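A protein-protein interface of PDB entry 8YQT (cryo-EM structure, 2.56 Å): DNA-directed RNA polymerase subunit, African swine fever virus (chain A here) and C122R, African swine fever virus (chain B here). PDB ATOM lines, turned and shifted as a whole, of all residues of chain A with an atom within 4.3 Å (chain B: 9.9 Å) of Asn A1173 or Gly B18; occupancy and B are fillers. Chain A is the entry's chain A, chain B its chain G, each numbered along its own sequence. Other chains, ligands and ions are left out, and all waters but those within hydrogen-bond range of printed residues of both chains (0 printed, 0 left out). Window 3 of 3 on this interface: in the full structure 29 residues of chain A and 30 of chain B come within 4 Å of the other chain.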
ATOM      1  N   LEU A1132     -15.205  31.573   5.947  1.00  0.00           N
ATOM      2  CA  LEU A1132     -14.119  30.643   5.691  1.00  0.00           C
ATOM      3  C   LEU A1132     -14.166  29.485   6.678  1.00  0.00           C
ATOM      4  O   LEU A1132     -14.417  29.671   7.872  1.00  0.00           O
ATOM      5  CB  LEU A1132     -12.763  31.350   5.783  1.00  0.00           C
ATOM      6  CG  LEU A1132     -12.606  32.587   4.899  1.00  0.00           C
ATOM      7  CD1 LEU A1132     -11.366  33.359   5.270  1.00  0.00           C
ATOM      8  CD2 LEU A1132     -12.548  32.186   3.447  1.00  0.00           C
ATOM      9  N   TYR A1133     -13.922  28.280   6.162  1.00  0.00           N
ATOM     10  CA  TYR A1133     -13.870  27.067   6.977  1.00  0.00           C
ATOM     11  C   TYR A1133     -12.422  26.870   7.416  1.00  0.00           C
ATOM     12  O   TYR A1133     -11.688  26.035   6.889  1.00  0.00           O
ATOM     13  CB  TYR A1133     -14.402  25.873   6.189  1.00  0.00           C
ATOM     14  CG  TYR A1133     -14.507  24.587   6.980  1.00  0.00           C
ATOM     15  CD1 TYR A1133     -15.577  24.359   7.834  1.00  0.00           C
ATOM     16  CD2 TYR A1133     -13.543  23.595   6.861  1.00  0.00           C
ATOM     17  CE1 TYR A1133     -15.679  23.185   8.553  1.00  0.00           C
ATOM     18  CE2 TYR A1133     -13.635  22.419   7.578  1.00  0.00           C
ATOM     19  CZ  TYR A1133     -14.705  22.220   8.421  1.00  0.00           C
ATOM     20  OH  TYR A1133     -14.799  21.049   9.135  1.00  0.00           O
ATOM     21  N   GLU A1134     -12.007  27.674   8.391  1.00  0.00           N
ATOM     22  CA  GLU A1134     -10.634  27.654   8.868  1.00  0.00           C
ATOM     23  C   GLU A1134     -10.612  27.682  10.388  1.00  0.00           C
ATOM     24  O   GLU A1134     -11.492  28.262  11.028  1.00  0.00           O
ATOM     25  CB  GLU A1134      -9.827  28.842   8.335  1.00  0.00           C
ATOM     26  CG  GLU A1134      -9.713  28.914   6.828  1.00  0.00           C
ATOM     27  CD  GLU A1134      -8.906  30.112   6.376  1.00  0.00           C
ATOM     28  OE1 GLU A1134      -8.371  30.825   7.248  1.00  0.00           O
ATOM     29  OE2 GLU A1134      -8.814  30.347   5.154  1.00  0.00           O
ATOM     30  N   THR A1135      -9.594  27.051  10.957  1.00  0.00           N
ATOM     31  CA  THR A1135      -9.314  27.150  12.378  1.00  0.00           C
ATOM     32  C   THR A1135      -8.169  28.136  12.586  1.00  0.00           C
ATOM     33  O   THR A1135      -7.706  28.797  11.654  1.00  0.00           O
ATOM     34  CB  THR A1135      -8.980  25.779  12.967  1.00  0.00           C
ATOM     35  OG1 THR A1135      -8.563  25.929  14.329  1.00  0.00           O
ATOM     36  CG2 THR A1135      -7.873  25.110  12.170  1.00  0.00           C
ATOM     37  N   ALA A1172     -13.264  26.850  16.655  1.00  0.00           N
ATOM     38  CA  ALA A1172     -13.818  25.929  15.677  1.00  0.00           C
ATOM     39  C   ALA A1172     -13.122  26.096  14.328  1.00  0.00           C
ATOM     40  O   ALA A1172     -12.185  26.883  14.170  1.00  0.00           O
ATOM     41  CB  ALA A1172     -15.323  26.145  15.538  1.00  0.00           C
ATOM     42  N   ASN A1173     -13.587  25.335  13.342  1.00  0.00           N
ATOM     43  CA  ASN A1173     -13.135  25.467  11.957  1.00  0.00           C
ATOM     44  C   ASN A1173     -14.020  26.436  11.180  1.00  0.00           C
ATOM     45  O   ASN A1173     -14.501  26.121  10.095  1.00  0.00           O
ATOM     46  CB  ASN A1173     -13.119  24.100  11.282  1.00  0.00           C
ATOM     47  CG  ASN A1173     -12.053  23.187  11.836  1.00  0.00           C
ATOM     48  OD1 ASN A1173     -10.878  23.538  11.871  1.00  0.00           O
ATOM     49  ND2 ASN A1173     -12.461  22.006  12.284  1.00  0.00           N
ATOM     50  N   TRP A1174     -14.241  27.630  11.722  1.00  0.00           N
ATOM     51  CA  TRP A1174     -15.134  28.590  11.089  1.00  0.00           C
ATOM     52  C   TRP A1174     -14.615  30.000  11.306  1.00  0.00           C
ATOM     53  O   TRP A1174     -14.438  30.434  12.448  1.00  0.00           O
ATOM     54  CB  TRP A1174     -16.558  28.460  11.633  1.00  0.00           C
ATOM     55  CG  TRP A1174     -17.183  27.150  11.304  1.00  0.00           C
ATOM     56  CD1 TRP A1174     -17.244  26.050  12.103  1.00  0.00           C
ATOM     57  CD2 TRP A1174     -17.831  26.794  10.080  1.00  0.00           C
ATOM     58  NE1 TRP A1174     -17.896  25.031  11.456  1.00  0.00           N
ATOM     59  CE2 TRP A1174     -18.266  25.462  10.210  1.00  0.00           C
ATOM     60  CE3 TRP A1174     -18.087  27.473   8.885  1.00  0.00           C
ATOM     61  CZ2 TRP A1174     -18.941  24.795   9.192  1.00  0.00           C
ATOM     62  CZ3 TRP A1174     -18.761  26.810   7.877  1.00  0.00           C
ATOM     63  CH2 TRP A1174     -19.179  25.486   8.036  1.00  0.00           C
ATOM     64  N   THR B  14     -19.584  18.583   2.188  1.00  0.00           N
ATOM     65  CA  THR B  14     -19.819  18.141   3.553  1.00  0.00           C
ATOM     66  C   THR B  14     -18.558  18.391   4.367  1.00  0.00           C
ATOM     67  O   THR B  14     -17.459  18.510   3.822  1.00  0.00           O
ATOM     68  CB  THR B  14     -20.208  16.654   3.628  1.00  0.00           C
ATOM     69  OG1 THR B  14     -19.151  15.849   3.090  1.00  0.00           O
ATOM     70  CG2 THR B  14     -21.486  16.391   2.846  1.00  0.00           C
ATOM     71  N   TYR B  15     -18.723  18.478   5.684  1.00  0.00           N
ATOM     72  CA  TYR B  15     -17.630  18.808   6.591  1.00  0.00           C
ATOM     73  C   TYR B  15     -17.457  17.672   7.588  1.00  0.00           C
ATOM     74  O   TYR B  15     -18.420  17.281   8.257  1.00  0.00           O
ATOM     75  CB  TYR B  15     -17.910  20.128   7.312  1.00  0.00           C
ATOM     76  CG  TYR B  15     -18.335  21.238   6.378  1.00  0.00           C
ATOM     77  CD1 TYR B  15     -17.395  22.032   5.739  1.00  0.00           C
ATOM     78  CD2 TYR B  15     -19.676  21.481   6.125  1.00  0.00           C
ATOM     79  CE1 TYR B  15     -17.780  23.042   4.879  1.00  0.00           C
ATOM     80  CE2 TYR B  15     -20.069  22.486   5.268  1.00  0.00           C
ATOM     81  CZ  TYR B  15     -19.119  23.263   4.648  1.00  0.00           C
ATOM     82  OH  TYR B  15     -19.511  24.266   3.794  1.00  0.00           O
ATOM     83  N   VAL B  16     -16.238  17.146   7.688  1.00  0.00           N
ATOM     84  CA  VAL B  16     -15.926  16.025   8.569  1.00  0.00           C
ATOM     85  C   VAL B  16     -14.517  16.211   9.114  1.00  0.00           C
ATOM     86  O   VAL B  16     -13.549  16.223   8.342  1.00  0.00           O
ATOM     87  CB  VAL B  16     -16.043  14.671   7.847  1.00  0.00           C
ATOM     88  CG1 VAL B  16     -15.401  13.571   8.673  1.00  0.00           C
ATOM     89  CG2 VAL B  16     -17.498  14.329   7.553  1.00  0.00           C
ATOM     90  N   ASP B  17     -14.403  16.347  10.439  1.00  0.00           N
ATOM     91  CA  ASP B  17     -13.118  16.314  11.147  1.00  0.00           C
ATOM     92  C   ASP B  17     -12.125  17.329  10.584  1.00  0.00           C
ATOM     93  O   ASP B  17     -10.959  17.018  10.331  1.00  0.00           O
ATOM     94  CB  ASP B  17     -12.525  14.904  11.131  1.00  0.00           C
ATOM     95  CG  ASP B  17     -13.512  13.850  11.594  1.00  0.00           C
ATOM     96  OD1 ASP B  17     -14.715  14.168  11.706  1.00  0.00           O
ATOM     97  OD2 ASP B  17     -13.086  12.702  11.842  1.00  0.00           O
ATOM     98  N   GLY B  18     -12.595  18.558  10.390  1.00  0.00           N
ATOM     99  CA  GLY B  18     -11.735  19.606   9.887  1.00  0.00           C
ATOM    100  C   GLY B  18     -11.393  19.500   8.421  1.00  0.00           C
ATOM    101  O   GLY B  18     -10.497  20.215   7.957  1.00  0.00           O
ATOM    102  N   ASN B  19     -12.071  18.629   7.678  1.00  0.00           N
ATOM    103  CA  ASN B  19     -11.859  18.461   6.250  1.00  0.00           C
ATOM    104  C   ASN B  19     -13.159  18.709   5.500  1.00  0.00           C
ATOM    105  O   ASN B  19     -14.251  18.428   6.001  1.00  0.00           O
ATOM    106  CB  ASN B  19     -11.339  17.057   5.918  1.00  0.00           C
ATOM    107  CG  ASN B  19      -9.835  16.955   6.021  1.00  0.00           C
ATOM    108  OD1 ASN B  19      -9.106  17.799   5.501  1.00  0.00           O
ATOM    109  ND2 ASN B  19      -9.356  15.914   6.693  1.00  0.00           N
ATOM    110  N   ILE B  20     -13.029  19.247   4.293  1.00  0.00           N
ATOM    111  CA  ILE B  20     -14.150  19.424   3.380  1.00  0.00           C
ATOM    112  C   ILE B  20     -14.115  18.274   2.385  1.00  0.00           C
ATOM    113  O   ILE B  20     -13.097  18.049   1.718  1.00  0.00           O
ATOM    114  CB  ILE B  20     -14.090  20.783   2.667  1.00  0.00           C
ATOM    115  CG1 ILE B  20     -14.764  21.857   3.516  1.00  0.00           C
ATOM    116  CG2 ILE B  20     -14.758  20.710   1.309  1.00  0.00           C
ATOM    117  CD1 ILE B  20     -14.430  23.265   3.100  1.00  0.00           C
ATOM    118  N   ILE B  21     -15.214  17.531   2.297  1.00  0.00           N
ATOM    119  CA  ILE B  21     -15.332  16.400   1.387  1.00  0.00           C
ATOM    120  C   ILE B  21     -16.435  16.704   0.387  1.00  0.00           C
ATOM    121  O   ILE B  21     -17.550  17.076   0.771  1.00  0.00           O
ATOM    122  CB  ILE B  21     -15.623  15.089   2.138  1.00  0.00           C
ATOM    123  CG1 ILE B  21     -14.616  14.883   3.267  1.00  0.00           C
ATOM    124  CG2 ILE B  21     -15.566  13.913   1.186  1.00  0.00           C
ATOM    125  CD1 ILE B  21     -15.182  14.148   4.443  1.00  0.00           C
ATOM    126  N   GLN B  31     -11.344  15.357  -1.783  1.00  0.00           N
ATOM    127  CA  GLN B  31     -10.983  16.285  -0.723  1.00  0.00           C
ATOM    128  C   GLN B  31     -10.483  17.586  -1.333  1.00  0.00           C
ATOM    129  O   GLN B  31      -9.654  17.575  -2.248  1.00  0.00           O
ATOM    130  CB  GLN B  31      -9.898  15.698   0.184  1.00  0.00           C
ATOM    131  CG  GLN B  31     -10.231  14.348   0.793  1.00  0.00           C
ATOM    132  CD  GLN B  31     -11.400  14.411   1.750  1.00  0.00           C
ATOM    133  OE1 GLN B  31     -11.618  15.421   2.415  1.00  0.00           O
ATOM    134  NE2 GLN B  31     -12.153  13.321   1.834  1.00  0.00           N
ATOM    135  N   GLY B  32     -10.994  18.707  -0.826  1.00  0.00           N
ATOM    136  CA  GLY B  32     -10.495  20.001  -1.251  1.00  0.00           C
ATOM    137  C   GLY B  32      -9.221  20.378  -0.517  1.00  0.00           C
ATOM    138  O   GLY B  32      -9.041  20.076   0.662  1.00  0.00           O
ATOM    139  N   ASP B  33      -8.315  21.043  -1.234  1.00  0.00           N
ATOM    140  CA  ASP B  33      -7.042  21.401  -0.622  1.00  0.00           C
ATOM    141  C   ASP B  33      -7.053  22.812  -0.046  1.00  0.00           C
ATOM    142  O   ASP B  33      -6.967  22.985   1.173  1.00  0.00           O
ATOM    143  CB  ASP B  33      -5.913  21.267  -1.647  1.00  0.00           C
ATOM    144  CG  ASP B  33      -4.550  21.583  -1.059  1.00  0.00           C
ATOM    145  OD1 ASP B  33      -4.003  20.731  -0.328  1.00  0.00           O
ATOM    146  OD2 ASP B  33      -4.022  22.683  -1.330  1.00  0.00           O
ATOM    147  N   ASN B  36     -11.266  25.470  -1.898  1.00  0.00           N
ATOM    148  CA  ASN B  36     -12.641  25.142  -1.553  1.00  0.00           C
ATOM    149  C   ASN B  36     -13.012  25.562  -0.137  1.00  0.00           C
ATOM    150  O   ASN B  36     -14.062  25.149   0.365  1.00  0.00           O
ATOM    151  CB  ASN B  36     -12.881  23.644  -1.744  1.00  0.00           C
ATOM    152  CG  ASN B  36     -12.833  23.231  -3.201  1.00  0.00           C
ATOM    153  OD1 ASN B  36     -12.011  22.408  -3.600  1.00  0.00           O
ATOM    154  ND2 ASN B  36     -13.716  23.807  -4.007  1.00  0.00           N
ATOM    155  N   LEU B  37     -12.185  26.374   0.516  1.00  0.00           N
ATOM    156  CA  LEU B  37     -12.479  26.862   1.864  1.00  0.00           C
ATOM    157  C   LEU B  37     -13.230  28.192   1.828  1.00  0.00           C
ATOM    158  O   LEU B  37     -12.840  29.163   2.468  1.00  0.00           O
ATOM    159  CB  LEU B  37     -11.186  26.988   2.659  1.00  0.00           C
ATOM    160  CG  LEU B  37     -10.364  25.715   2.860  1.00  0.00           C
ATOM    161  CD1 LEU B  37      -9.055  26.032   3.559  1.00  0.00           C
ATOM    162  CD2 LEU B  37     -11.149  24.683   3.640  1.00  0.00           C
ATOM    163  N   LEU B  38     -14.325  28.242   1.072  1.00  0.00           N
ATOM    164  CA  LEU B  38     -15.161  29.439   0.970  1.00  0.00           C
ATOM    165  C   LEU B  38     -16.616  28.993   1.039  1.00  0.00           C
ATOM    166  O   LEU B  38     -17.207  28.625   0.021  1.00  0.00           O
ATOM    167  CB  LEU B  38     -14.882  30.212  -0.312  1.00  0.00           C
ATOM    168  CG  LEU B  38     -15.397  31.654  -0.355  1.00  0.00           C
ATOM    169  CD1 LEU B  38     -14.842  32.474   0.791  1.00  0.00           C
ATOM    170  CD2 LEU B  38     -15.068  32.304  -1.687  1.00  0.00           C
ATOM    171  N   VAL B  39     -17.187  29.030   2.240  1.00  0.00           N
ATOM    172  CA  VAL B  39     -18.556  28.568   2.427  1.00  0.00           C
ATOM    173  C   VAL B  39     -19.545  29.513   1.759  1.00  0.00           C
ATOM    174  O   VAL B  39     -20.430  29.082   1.012  1.00  0.00           O
ATOM    175  CB  VAL B  39     -18.857  28.407   3.928  1.00  0.00           C
ATOM    176  CG1 VAL B  39     -20.226  27.785   4.127  1.00  0.00           C
ATOM    177  CG2 VAL B  39     -17.772  27.580   4.593  1.00  0.00           C
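Asn A1173 touches just one residue of chain B: Gly B18. Of chain A, only Tyr A1133 and Asn A1173 come within 4 Å of Gly B18. Tyr A1133 touches just these residues of chain B: Tyr B15 (3.5 Å), Gly B18 (3.5 Å), Asn B19 (3.9 Å), Ile B20 (3.9 Å) and Leu B37 (3.6 Å). No residue of chain B comes within 4 Å of Ala A1172. Of chain B, only Val B39 (3.5 Å) comes within 4 Å of Trp A1174. Of the printed residues of chain A, Leu B37 touches Leu A1132 (3.2 Å) and Tyr A1133 (3.6 Å). Of the printed residues of chain A, Tyr B15 touches Tyr A1133. Printed residues of chain A within 4 Å of Ile B20: Tyr A1133 (3.9 Å). Of the printed residues of chain B, Leu A1132 touches Leu B37 (3.2 Å) and Leu B38 (3.5 Å). Ile B21 touches none of the printed residues of chain A. The nearest printed residue of chain A that does not touch Gly B18 is Thr A1135 (7.0 Å).
Hydrophobic or aromatic side chains of chain B within 4 Å of the printed part of chain A: Tyr B15, Ile B20, Leu B37, Leu B38 and Val B39. Among the printed residues, 9 pairs touch across the chains. Among the printed residues, no Asp or Glu carboxylate lies within 4 Å of a Lys or Arg side-chain nitrogen of the other chain.
The backbone NH of Glu A1134 lies within hydrogen-bond range of the backbone carbonyl oxygen of Asn A1173, 3.4 Å away. The backbone NH of Trp A1174 sits at hydrogen-bond distance from the backbone carbonyl oxygen of Glu A1134 (2.9 Å). The backbone carbonyl oxygen of Ile B20 sits close to the side-chain amide oxygen of Gln B31, 3.1 Å away. The backbone NH (N) of Gly B32 sits at hydrogen-bond distance from the backbone carbonyl oxygen (O) of Ile B20, at 3.4 Å.
O of Leu B37 touches CD2 of Leu A1132, at 3.2 Å. CD2 of Leu A1132 touches CD1 of Leu B38, 3.5 Å away. CE1 of Tyr A1133 touches CD1 of Tyr B15, 3.5 Å away. OH of Tyr A1133 touches CA of Gly B18 (3.5 Å). Tyr A1133 touches Asn B19. Tyr A1133 touches Ile B20. O of Tyr A1133 touches CD2 of Leu B37, 3.6 Å away. Gly B18 touches Asn A1173 (CA to ND2, 3.5 Å). Trp A1174 touches Val B39 (CZ3 to CG2, 3.5 Å).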
